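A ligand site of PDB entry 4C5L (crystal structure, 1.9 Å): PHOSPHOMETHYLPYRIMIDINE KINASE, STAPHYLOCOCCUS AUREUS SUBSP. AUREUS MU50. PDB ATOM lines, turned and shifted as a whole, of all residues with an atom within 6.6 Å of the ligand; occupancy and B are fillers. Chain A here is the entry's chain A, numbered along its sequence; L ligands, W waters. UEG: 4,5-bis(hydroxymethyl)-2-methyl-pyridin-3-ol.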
ATOM      1  N   ALA A  10     -27.005   0.139 -20.970  1.00  0.00           N
ATOM      2  CA  ALA A  10     -27.340   0.162 -19.567  1.00  0.00           C
ATOM      3  C   ALA A  10     -27.209   1.558 -19.022  1.00  0.00           C
ATOM      4  O   ALA A  10     -26.745   2.454 -19.694  1.00  0.00           O
ATOM      5  CB  ALA A  10     -26.404  -0.796 -18.817  1.00  0.00           C
ATOM      6  N   GLY A  11     -27.564   1.695 -17.747  1.00  0.00           N
ATOM      7  CA  GLY A  11     -27.388   2.921 -17.018  1.00  0.00           C
ATOM      8  C   GLY A  11     -26.212   2.877 -16.086  1.00  0.00           C
ATOM      9  O   GLY A  11     -25.636   1.797 -15.792  1.00  0.00           O
ATOM     10  N   SER A  12     -25.864   4.056 -15.613  1.00  0.00           N
ATOM     11  CA  SER A  12     -24.843   4.181 -14.577  1.00  0.00           C
ATOM     12  C   SER A  12     -25.461   4.047 -13.206  1.00  0.00           C
ATOM     13  O   SER A  12     -26.348   4.816 -12.814  1.00  0.00           O
ATOM     14  CB  SER A  12     -24.127   5.521 -14.705  1.00  0.00           C
ATOM     15  OG  SER A  12     -23.239   5.664 -13.626  1.00  0.00           O
ATOM     16  N   ASP A  13     -24.973   3.044 -12.480  1.00  0.00           N
ATOM     17  CA  ASP A  13     -25.192   2.927 -11.063  1.00  0.00           C
ATOM     18  C   ASP A  13     -24.052   3.670 -10.366  1.00  0.00           C
ATOM     19  O   ASP A  13     -22.971   3.132 -10.159  1.00  0.00           O
ATOM     20  CB  ASP A  13     -25.178   1.456 -10.621  1.00  0.00           C
ATOM     21  CG  ASP A  13     -24.987   1.298  -9.120  1.00  0.00           C
ATOM     22  OD1 ASP A  13     -25.270   2.286  -8.408  1.00  0.00           O
ATOM     23  OD2 ASP A  13     -24.555   0.222  -8.662  1.00  0.00           O
ATOM     24  N   THR A  14     -24.297   4.912  -9.974  1.00  0.00           N
ATOM     25  CA  THR A  14     -23.265   5.658  -9.314  1.00  0.00           C
ATOM     26  C   THR A  14     -22.560   4.883  -8.199  1.00  0.00           C
ATOM     27  O   THR A  14     -21.345   5.017  -8.075  1.00  0.00           O
ATOM     28  CB  THR A  14     -23.794   6.996  -8.799  1.00  0.00           C
ATOM     29  OG1 THR A  14     -24.365   7.716  -9.905  1.00  0.00           O
ATOM     30  CG2 THR A  14     -22.645   7.783  -8.147  1.00  0.00           C
ATOM     31  N   SER A  15     -23.300   4.088  -7.406  1.00  0.00           N
ATOM     32  CA  SER A  15     -22.687   3.289  -6.331  1.00  0.00           C
ATOM     33  C   SER A  15     -21.681   2.244  -6.855  1.00  0.00           C
ATOM     34  O   SER A  15     -20.882   1.753  -6.103  1.00  0.00           O
ATOM     35  CB  SER A  15     -23.744   2.606  -5.409  1.00  0.00           C
ATOM     36  OG  SER A  15     -24.452   1.572  -6.084  1.00  0.00           O
ATOM     37  N   ALA A  18     -23.752  -2.207  -9.449  1.00  0.00           N
ATOM     38  CA  ALA A  18     -24.615  -2.763 -10.458  1.00  0.00           C
ATOM     39  C   ALA A  18     -24.486  -1.937 -11.739  1.00  0.00           C
ATOM     40  O   ALA A  18     -23.552  -1.198 -11.887  1.00  0.00           O
ATOM     41  CB  ALA A  18     -26.053  -2.763  -9.961  1.00  0.00           C
ATOM     42  N   GLY A  19     -25.397  -2.119 -12.670  1.00  0.00           N
ATOM     43  CA  GLY A  19     -25.475  -1.279 -13.870  1.00  0.00           C
ATOM     44  C   GLY A  19     -24.249  -1.445 -14.723  1.00  0.00           C
ATOM     45  O   GLY A  19     -23.599  -2.527 -14.726  1.00  0.00           O
ATOM     46  N   MET A  20     -23.912  -0.395 -15.466  1.00  0.00           N
ATOM     47  CA  MET A  20     -22.769  -0.471 -16.374  1.00  0.00           C
ATOM     48  C   MET A  20     -21.451  -0.676 -15.673  1.00  0.00           C
ATOM     49  O   MET A  20     -20.570  -1.300 -16.212  1.00  0.00           O
ATOM     50  CB  MET A  20     -22.708   0.711 -17.308  1.00  0.00           C
ATOM     51  CG  MET A  20     -22.406   2.023 -16.632  1.00  0.00           C
ATOM     52  SD  MET A  20     -20.654   2.384 -16.690  1.00  0.00           S
ATOM     53  CE  MET A  20     -20.682   3.930 -15.816  1.00  0.00           C
ATOM     54  N   GLN A  21     -21.357  -0.208 -14.428  1.00  0.00           N
ATOM     55  CA  GLN A  21     -20.175  -0.405 -13.669  1.00  0.00           C
ATOM     56  C   GLN A  21     -19.927  -1.902 -13.473  1.00  0.00           C
ATOM     57  O   GLN A  21     -18.799  -2.402 -13.718  1.00  0.00           O
ATOM     58  CB  GLN A  21     -20.244   0.333 -12.340  1.00  0.00           C
ATOM     59  CG  GLN A  21     -20.157   1.849 -12.404  1.00  0.00           C
ATOM     60  CD  GLN A  21     -21.454   2.568 -12.822  1.00  0.00           C
ATOM     61  OE1 GLN A  21     -22.419   1.945 -13.293  1.00  0.00           O
ATOM     62  NE2 GLN A  21     -21.450   3.889 -12.697  1.00  0.00           N
ATOM     63  N   THR A  39     -27.772   4.865 -20.897  1.00  0.00           N
ATOM     64  CA  THR A  39     -29.193   5.217 -20.999  1.00  0.00           C
ATOM     65  C   THR A  39     -29.647   6.187 -19.949  1.00  0.00           C
ATOM     66  O   THR A  39     -30.588   6.925 -20.151  1.00  0.00           O
ATOM     67  CB  THR A  39     -30.085   3.970 -20.857  1.00  0.00           C
ATOM     68  OG1 THR A  39     -29.817   3.325 -19.611  1.00  0.00           O
ATOM     69  CG2 THR A  39     -29.805   3.026 -22.010  1.00  0.00           C
ATOM     70  N   ALA A  40     -28.993   6.173 -18.799  1.00  0.00           N
ATOM     71  CA  ALA A  40     -29.433   6.962 -17.715  1.00  0.00           C
ATOM     72  C   ALA A  40     -28.364   6.962 -16.665  1.00  0.00           C
ATOM     73  O   ALA A  40     -27.424   6.147 -16.711  1.00  0.00           O
ATOM     74  CB  ALA A  40     -30.737   6.404 -17.131  1.00  0.00           C
ATOM     75  N   ILE A  41     -28.535   7.869 -15.705  1.00  0.00           N
ATOM     76  CA  ILE A  41     -27.666   7.955 -14.555  1.00  0.00           C
ATOM     77  C   ILE A  41     -28.438   7.842 -13.266  1.00  0.00           C
ATOM     78  O   ILE A  41     -29.284   8.672 -12.989  1.00  0.00           O
ATOM     79  CB  ILE A  41     -26.916   9.291 -14.601  1.00  0.00           C
ATOM     80  CG1 ILE A  41     -26.051   9.289 -15.861  1.00  0.00           C
ATOM     81  CG2 ILE A  41     -26.155   9.528 -13.302  1.00  0.00           C
ATOM     82  CD1 ILE A  41     -25.176  10.488 -15.998  1.00  0.00           C
ATOM     83  N   VAL A  42     -28.145   6.803 -12.488  1.00  0.00           N
ATOM     84  CA  VAL A  42     -28.835   6.563 -11.238  1.00  0.00           C
ATOM     85  C   VAL A  42     -27.966   7.047 -10.093  1.00  0.00           C
ATOM     86  O   VAL A  42     -26.816   6.667  -9.989  1.00  0.00           O
ATOM     87  CB  VAL A  42     -29.148   5.074 -10.992  1.00  0.00           C
ATOM     88  CG1 VAL A  42     -29.935   4.888  -9.701  1.00  0.00           C
ATOM     89  CG2 VAL A  42     -29.908   4.484 -12.164  1.00  0.00           C
ATOM     90  N   MET A  44     -28.095   8.217  -5.680  1.00  0.00           N
ATOM     91  CA  MET A  44     -28.699   7.794  -4.453  1.00  0.00           C
ATOM     92  C   MET A  44     -28.442   8.855  -3.426  1.00  0.00           C
ATOM     93  O   MET A  44     -27.327   9.349  -3.322  1.00  0.00           O
ATOM     94  CB  MET A  44     -28.119   6.447  -3.995  1.00  0.00           C
ATOM     95  CG  MET A  44     -28.346   5.286  -4.961  1.00  0.00           C
ATOM     96  SD  MET A  44     -27.164   5.099  -6.297  1.00  0.00           S
ATOM     97  CE  MET A  44     -27.918   3.683  -7.116  1.00  0.00           C
ATOM     98  N   HIS A  51     -33.391   6.244  -4.713  1.00  0.00           N
ATOM     99  CA  HIS A  51     -32.876   6.258  -6.073  1.00  0.00           C
ATOM    100  C   HIS A  51     -33.476   7.383  -6.892  1.00  0.00           C
ATOM    101  O   HIS A  51     -34.658   7.604  -6.852  1.00  0.00           O
ATOM    102  CB  HIS A  51     -33.158   4.933  -6.757  1.00  0.00           C
ATOM    103  CG  HIS A  51     -32.254   3.838  -6.298  1.00  0.00           C
ATOM    104  ND1 HIS A  51     -31.782   3.748  -5.000  1.00  0.00           N
ATOM    105  CD2 HIS A  51     -31.717   2.790  -6.964  1.00  0.00           C
ATOM    106  CE1 HIS A  51     -30.991   2.694  -4.893  1.00  0.00           C
ATOM    107  NE2 HIS A  51     -30.929   2.104  -6.068  1.00  0.00           N
ATOM    108  N   GLY A  79     -29.285  -3.882 -19.906  1.00  0.00           N
ATOM    109  CA  GLY A  79     -29.579  -3.654 -18.494  1.00  0.00           C
ATOM    110  C   GLY A  79     -30.772  -2.696 -18.467  1.00  0.00           C
ATOM    111  O   GLY A  79     -31.820  -2.976 -19.026  1.00  0.00           O
ATOM    112  N   MET A  80     -30.585  -1.560 -17.826  1.00  0.00           N
ATOM    113  CA  MET A  80     -31.675  -0.618 -17.611  1.00  0.00           C
ATOM    114  C   MET A  80     -31.885   0.172 -18.841  1.00  0.00           C
ATOM    115  O   MET A  80     -30.950   0.798 -19.374  1.00  0.00           O
ATOM    116  CB  MET A  80     -31.375   0.338 -16.482  1.00  0.00           C
ATOM    117  CG  MET A  80     -32.384   1.497 -16.369  1.00  0.00           C
ATOM    118  SD  MET A  80     -31.956   2.491 -14.913  1.00  0.00           S
ATOM    119  CE  MET A  80     -32.524   1.415 -13.606  1.00  0.00           C
ATOM    120  N   ASP A 105     -31.070  -8.730 -19.551  1.00  0.00           N
ATOM    121  CA  ASP A 105     -31.349  -8.719 -18.148  1.00  0.00           C
ATOM    122  C   ASP A 105     -32.497  -7.711 -18.054  1.00  0.00           C
ATOM    123  O   ASP A 105     -32.280  -6.486 -18.195  1.00  0.00           O
ATOM    124  CB  ASP A 105     -30.125  -8.273 -17.335  1.00  0.00           C
ATOM    125  CG  ASP A 105     -30.403  -8.249 -15.842  1.00  0.00           C
ATOM    126  OD1 ASP A 105     -31.445  -8.869 -15.431  1.00  0.00           O
ATOM    127  OD2 ASP A 105     -29.619  -7.626 -15.079  1.00  0.00           O
ATOM    128  N   VAL A 107     -34.200  -5.649 -16.365  1.00  0.00           N
ATOM    129  CA  VAL A 107     -34.197  -4.982 -15.071  1.00  0.00           C
ATOM    130  C   VAL A 107     -35.409  -4.077 -14.911  1.00  0.00           C
ATOM    131  O   VAL A 107     -35.786  -3.285 -15.830  1.00  0.00           O
ATOM    132  CB  VAL A 107     -32.862  -4.279 -14.665  1.00  0.00           C
ATOM    133  CG1 VAL A 107     -31.763  -4.404 -15.734  1.00  0.00           C
ATOM    134  CG2 VAL A 107     -33.090  -2.845 -14.206  1.00  0.00           C
ATOM    135  N   MET A 108     -36.021  -4.258 -13.736  1.00  0.00           N
ATOM    136  CA  MET A 108     -37.198  -3.529 -13.295  1.00  0.00           C
ATOM    137  C   MET A 108     -36.986  -2.973 -11.885  1.00  0.00           C
ATOM    138  O   MET A 108     -37.601  -1.961 -11.528  1.00  0.00           O
ATOM    139  CB  MET A 108     -38.429  -4.459 -13.324  1.00  0.00           C
ATOM    140  CG  MET A 108     -38.836  -4.913 -14.724  1.00  0.00           C
ATOM    141  SD  MET A 108     -40.260  -6.054 -14.804  1.00  0.00           S
ATOM    142  CE  MET A 108     -40.151  -6.568 -16.527  1.00  0.00           C
ATOM    143  N   VAL A 109     -36.122  -3.606 -11.082  1.00  0.00           N
ATOM    144  CA  VAL A 109     -35.849  -3.176  -9.700  1.00  0.00           C
ATOM    145  C   VAL A 109     -34.357  -3.315  -9.352  1.00  0.00           C
ATOM    146  O   VAL A 109     -33.617  -4.174  -9.887  1.00  0.00           O
ATOM    147  CB  VAL A 109     -36.655  -3.967  -8.623  1.00  0.00           C
ATOM    148  CG1 VAL A 109     -36.698  -3.208  -7.280  1.00  0.00           C
ATOM    149  CG2 VAL A 109     -38.083  -4.238  -9.080  1.00  0.00           C
ATOM    150  N   CYS A 110     -33.934  -2.432  -8.449  1.00  0.00           N
ATOM    151  CA  CYS A 110     -32.598  -2.336  -7.934  1.00  0.00           C
ATOM    152  C   CYS A 110     -32.606  -2.732  -6.476  1.00  0.00           C
ATOM    153  O   CYS A 110     -33.544  -2.428  -5.721  1.00  0.00           O
ATOM    154  CB  CYS A 110     -32.113  -0.882  -8.012  1.00  0.00           C
ATOM    155  SG  CYS A 110     -31.558  -0.496  -9.632  1.00  0.00           S
ATOM    156  N   LYS A 111     -31.529  -3.396  -6.073  1.00  0.00           N
ATOM    157  CA  LYS A 111     -31.304  -3.672  -4.684  1.00  0.00           C
ATOM    158  C   LYS A 111     -31.244  -2.307  -3.969  1.00  0.00           C
ATOM    159  O   LYS A 111     -30.621  -1.365  -4.465  1.00  0.00           O
ATOM    160  CB  LYS A 111     -30.009  -4.515  -4.543  1.00  0.00           C
ATOM    161  CG  LYS A 111     -30.140  -5.877  -5.245  1.00  0.00           C
ATOM    162  CD  LYS A 111     -29.047  -6.209  -6.281  1.00  0.00           C
ATOM    163  CE  LYS A 111     -29.210  -5.622  -7.694  1.00  0.00           C
ATOM    164  NZ  LYS A 111     -28.665  -6.429  -8.840  1.00  0.00           N
ATOM    165  N   GLU A 142     -39.418 -10.249 -12.018  1.00  0.00           N
ATOM    166  CA  GLU A 142     -39.399  -9.865 -13.410  1.00  0.00           C
ATOM    167  C   GLU A 142     -39.954 -11.008 -14.239  1.00  0.00           C
ATOM    168  O   GLU A 142     -40.681 -10.773 -15.211  1.00  0.00           O
ATOM    169  CB  GLU A 142     -37.985  -9.476 -13.835  1.00  0.00           C
ATOM    170  CG  GLU A 142     -37.466  -8.161 -13.203  1.00  0.00           C
ATOM    171  CD  GLU A 142     -35.945  -8.084 -13.016  1.00  0.00           C
ATOM    172  OE1 GLU A 142     -35.246  -9.134 -13.125  1.00  0.00           O
ATOM    173  OE2 GLU A 142     -35.445  -6.945 -12.717  1.00  0.00           O
ATOM    174  N   HIS A 210     -25.795  -6.724  -3.972  1.00  0.00           N
ATOM    175  CA  HIS A 210     -26.054  -5.628  -4.905  1.00  0.00           C
ATOM    176  C   HIS A 210     -25.191  -5.782  -6.171  1.00  0.00           C
ATOM    177  O   HIS A 210     -23.971  -5.885  -6.102  1.00  0.00           O
ATOM    178  CB  HIS A 210     -25.839  -4.281  -4.245  1.00  0.00           C
ATOM    179  CG  HIS A 210     -25.872  -3.133  -5.206  1.00  0.00           C
ATOM    180  ND1 HIS A 210     -26.876  -2.954  -6.125  1.00  0.00           N
ATOM    181  CD2 HIS A 210     -25.014  -2.092  -5.378  1.00  0.00           C
ATOM    182  CE1 HIS A 210     -26.664  -1.837  -6.808  1.00  0.00           C
ATOM    183  NE2 HIS A 210     -25.548  -1.290  -6.364  1.00  0.00           N
ATOM    184  N   GLY A 211     -25.875  -5.810  -7.307  1.00  0.00           N
ATOM    185  CA  GLY A 211     -25.281  -6.051  -8.615  1.00  0.00           C
ATOM    186  C   GLY A 211     -25.155  -7.526  -9.004  1.00  0.00           C
ATOM    187  O   GLY A 211     -24.543  -7.844 -10.040  1.00  0.00           O
ATOM    188  N   ALA A 212     -25.744  -8.432  -8.229  1.00  0.00           N
ATOM    189  CA  ALA A 212     -25.612  -9.873  -8.555  1.00  0.00           C
ATOM    190  C   ALA A 212     -26.237 -10.188  -9.942  1.00  0.00           C
ATOM    191  O   ALA A 212     -25.637 -10.892 -10.746  1.00  0.00           O
ATOM    192  CB  ALA A 212     -26.222 -10.731  -7.489  1.00  0.00           C
ATOM    193  N   GLY A 213     -27.402  -9.641 -10.221  1.00  0.00           N
ATOM    194  CA  GLY A 213     -28.082  -9.902 -11.497  1.00  0.00           C
ATOM    195  C   GLY A 213     -27.341  -9.367 -12.712  1.00  0.00           C
ATOM    196  O   GLY A 213     -27.210 -10.040 -13.720  1.00  0.00           O
ATOM    197  N   CYS A 214     -26.862  -8.120 -12.612  1.00  0.00           N
ATOM    198  CA  CYS A 214     -26.088  -7.486 -13.682  1.00  0.00           C
ATOM    199  C   CYS A 214     -24.792  -8.265 -13.916  1.00  0.00           C
ATOM    200  O   CYS A 214     -24.418  -8.552 -15.052  1.00  0.00           O
ATOM    201  CB  CYS A 214     -25.772  -6.036 -13.279  1.00  0.00           C
ATOM    202  SG  CYS A 214     -27.209  -4.928 -13.220  1.00  0.00           S
HETATM  203  OP4 UEG L   1     -29.519  -4.073 -10.570  1.00  0.00           O
HETATM  204  C5A UEG L   1     -30.354  -3.369 -11.510  1.00  0.00           C
HETATM  205  C5  UEG L   1     -29.736  -2.054 -11.950  1.00  0.00           C
HETATM  206  C6  UEG L   1     -29.350  -1.929 -13.306  1.00  0.00           C
HETATM  207  N1  UEG L   1     -28.812  -0.800 -13.811  1.00  0.00           N
HETATM  208  C2  UEG L   1     -28.609   0.275 -13.017  1.00  0.00           C
HETATM  209  C3  UEG L   1     -28.943   0.191 -11.687  1.00  0.00           C
HETATM  210  C4  UEG L   1     -29.457  -0.961 -11.144  1.00  0.00           C
HETATM  211  C4A UEG L   1     -29.867  -0.733  -9.758  1.00  0.00           C
HETATM  212  O4A UEG L   1     -29.067  -0.456  -8.839  1.00  0.00           O
HETATM  213  O3  UEG L   1     -28.729   1.288 -10.889  1.00  0.00           O
HETATM  214  C2A UEG L   1     -27.980   1.531 -13.565  1.00  0.00           C
HETATM  215  O   HOH W   1     -28.275  -1.068 -16.207  1.00  0.00           O
HETATM  216  O   HOH W   2     -29.181  -0.018  -6.204  1.00  0.00           O
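The side-chain amino group (NZ) of Lys 111 is in hydrogen-bond range of an oxygen (OP4) of the ligand (3.0 Å).
The side-chain sulfur of Cys 110 is bonded to a carbon (C4A) of the ligand (1.7 Å).
The side-chain sulfur (SG) of Cys 214 is in hydrogen-bond range of an oxygen (OP4) of the ligand (3.6 Å).
The backbone NH of Asp 13 is in hydrogen-bond range of the side-chain amide oxygen of Gln 21 (2.9 Å).
The backbone carbonyl oxygen of Met 80 lies within hydrogen-bond range of the side-chain hydroxyl of Thr 39.
The side-chain hydroxyl (OG) of Ser 12 lies within hydrogen-bond range of the side-chain amide nitrogen (NE2) of Gln 21.
The side-chain carboxylate (OD2) of Asp 13 sits at hydrogen-bond distance from the backbone NH (N) of Ala 18 (2.7 Å).
O of Ser 12 is in hydrogen-bond range of N of Val 42.
The side-chain sulfur (SG) of Cys 214 lies within hydrogen-bond range of the backbone NH (N) of Gly 19, at 3.4 Å.
OG of Ser 15 sits at hydrogen-bond distance from NE2 of His 210, at 3.1 Å.
The backbone carbonyl oxygen of Gly 11 sits at hydrogen-bond distance from the backbone NH of Met 20 (2.8 Å).
O of Gly 11 touches C2A of the ligand (3.2 Å).
Ser 12 touches the ligand (C to C2A, 3.6 Å).
Asp 13 touches the ligand.
Ala 18 touches the ligand.
Gly 19 touches the ligand.
Val 42 touches the ligand (CG2 to O3, 3.6 Å).
Met 80 touches the ligand (CB to N1, 3.9 Å).
CG2 of Val 107 touches C5A of the ligand (3.9 Å).
O of Val 109 touches C5A of the ligand (3.7 Å).
CE1 of His 210 touches O4A of the ligand, 3.4 Å away.
The nearest printed residue that does not touch the ligand is His 51 (4.2 Å).
Water W1 lies within hydrogen-bond range of N1 of the ligand (2.5 Å), N of Met 80 (2.9 Å) and N of Gly 11 (3.2 Å).
Water W2 lies within hydrogen-bond range of the backbone carbonyl oxygen (O) of Lys 111, an oxygen (O4A) of the ligand and a ring nitrogen (NE2) of His 51.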
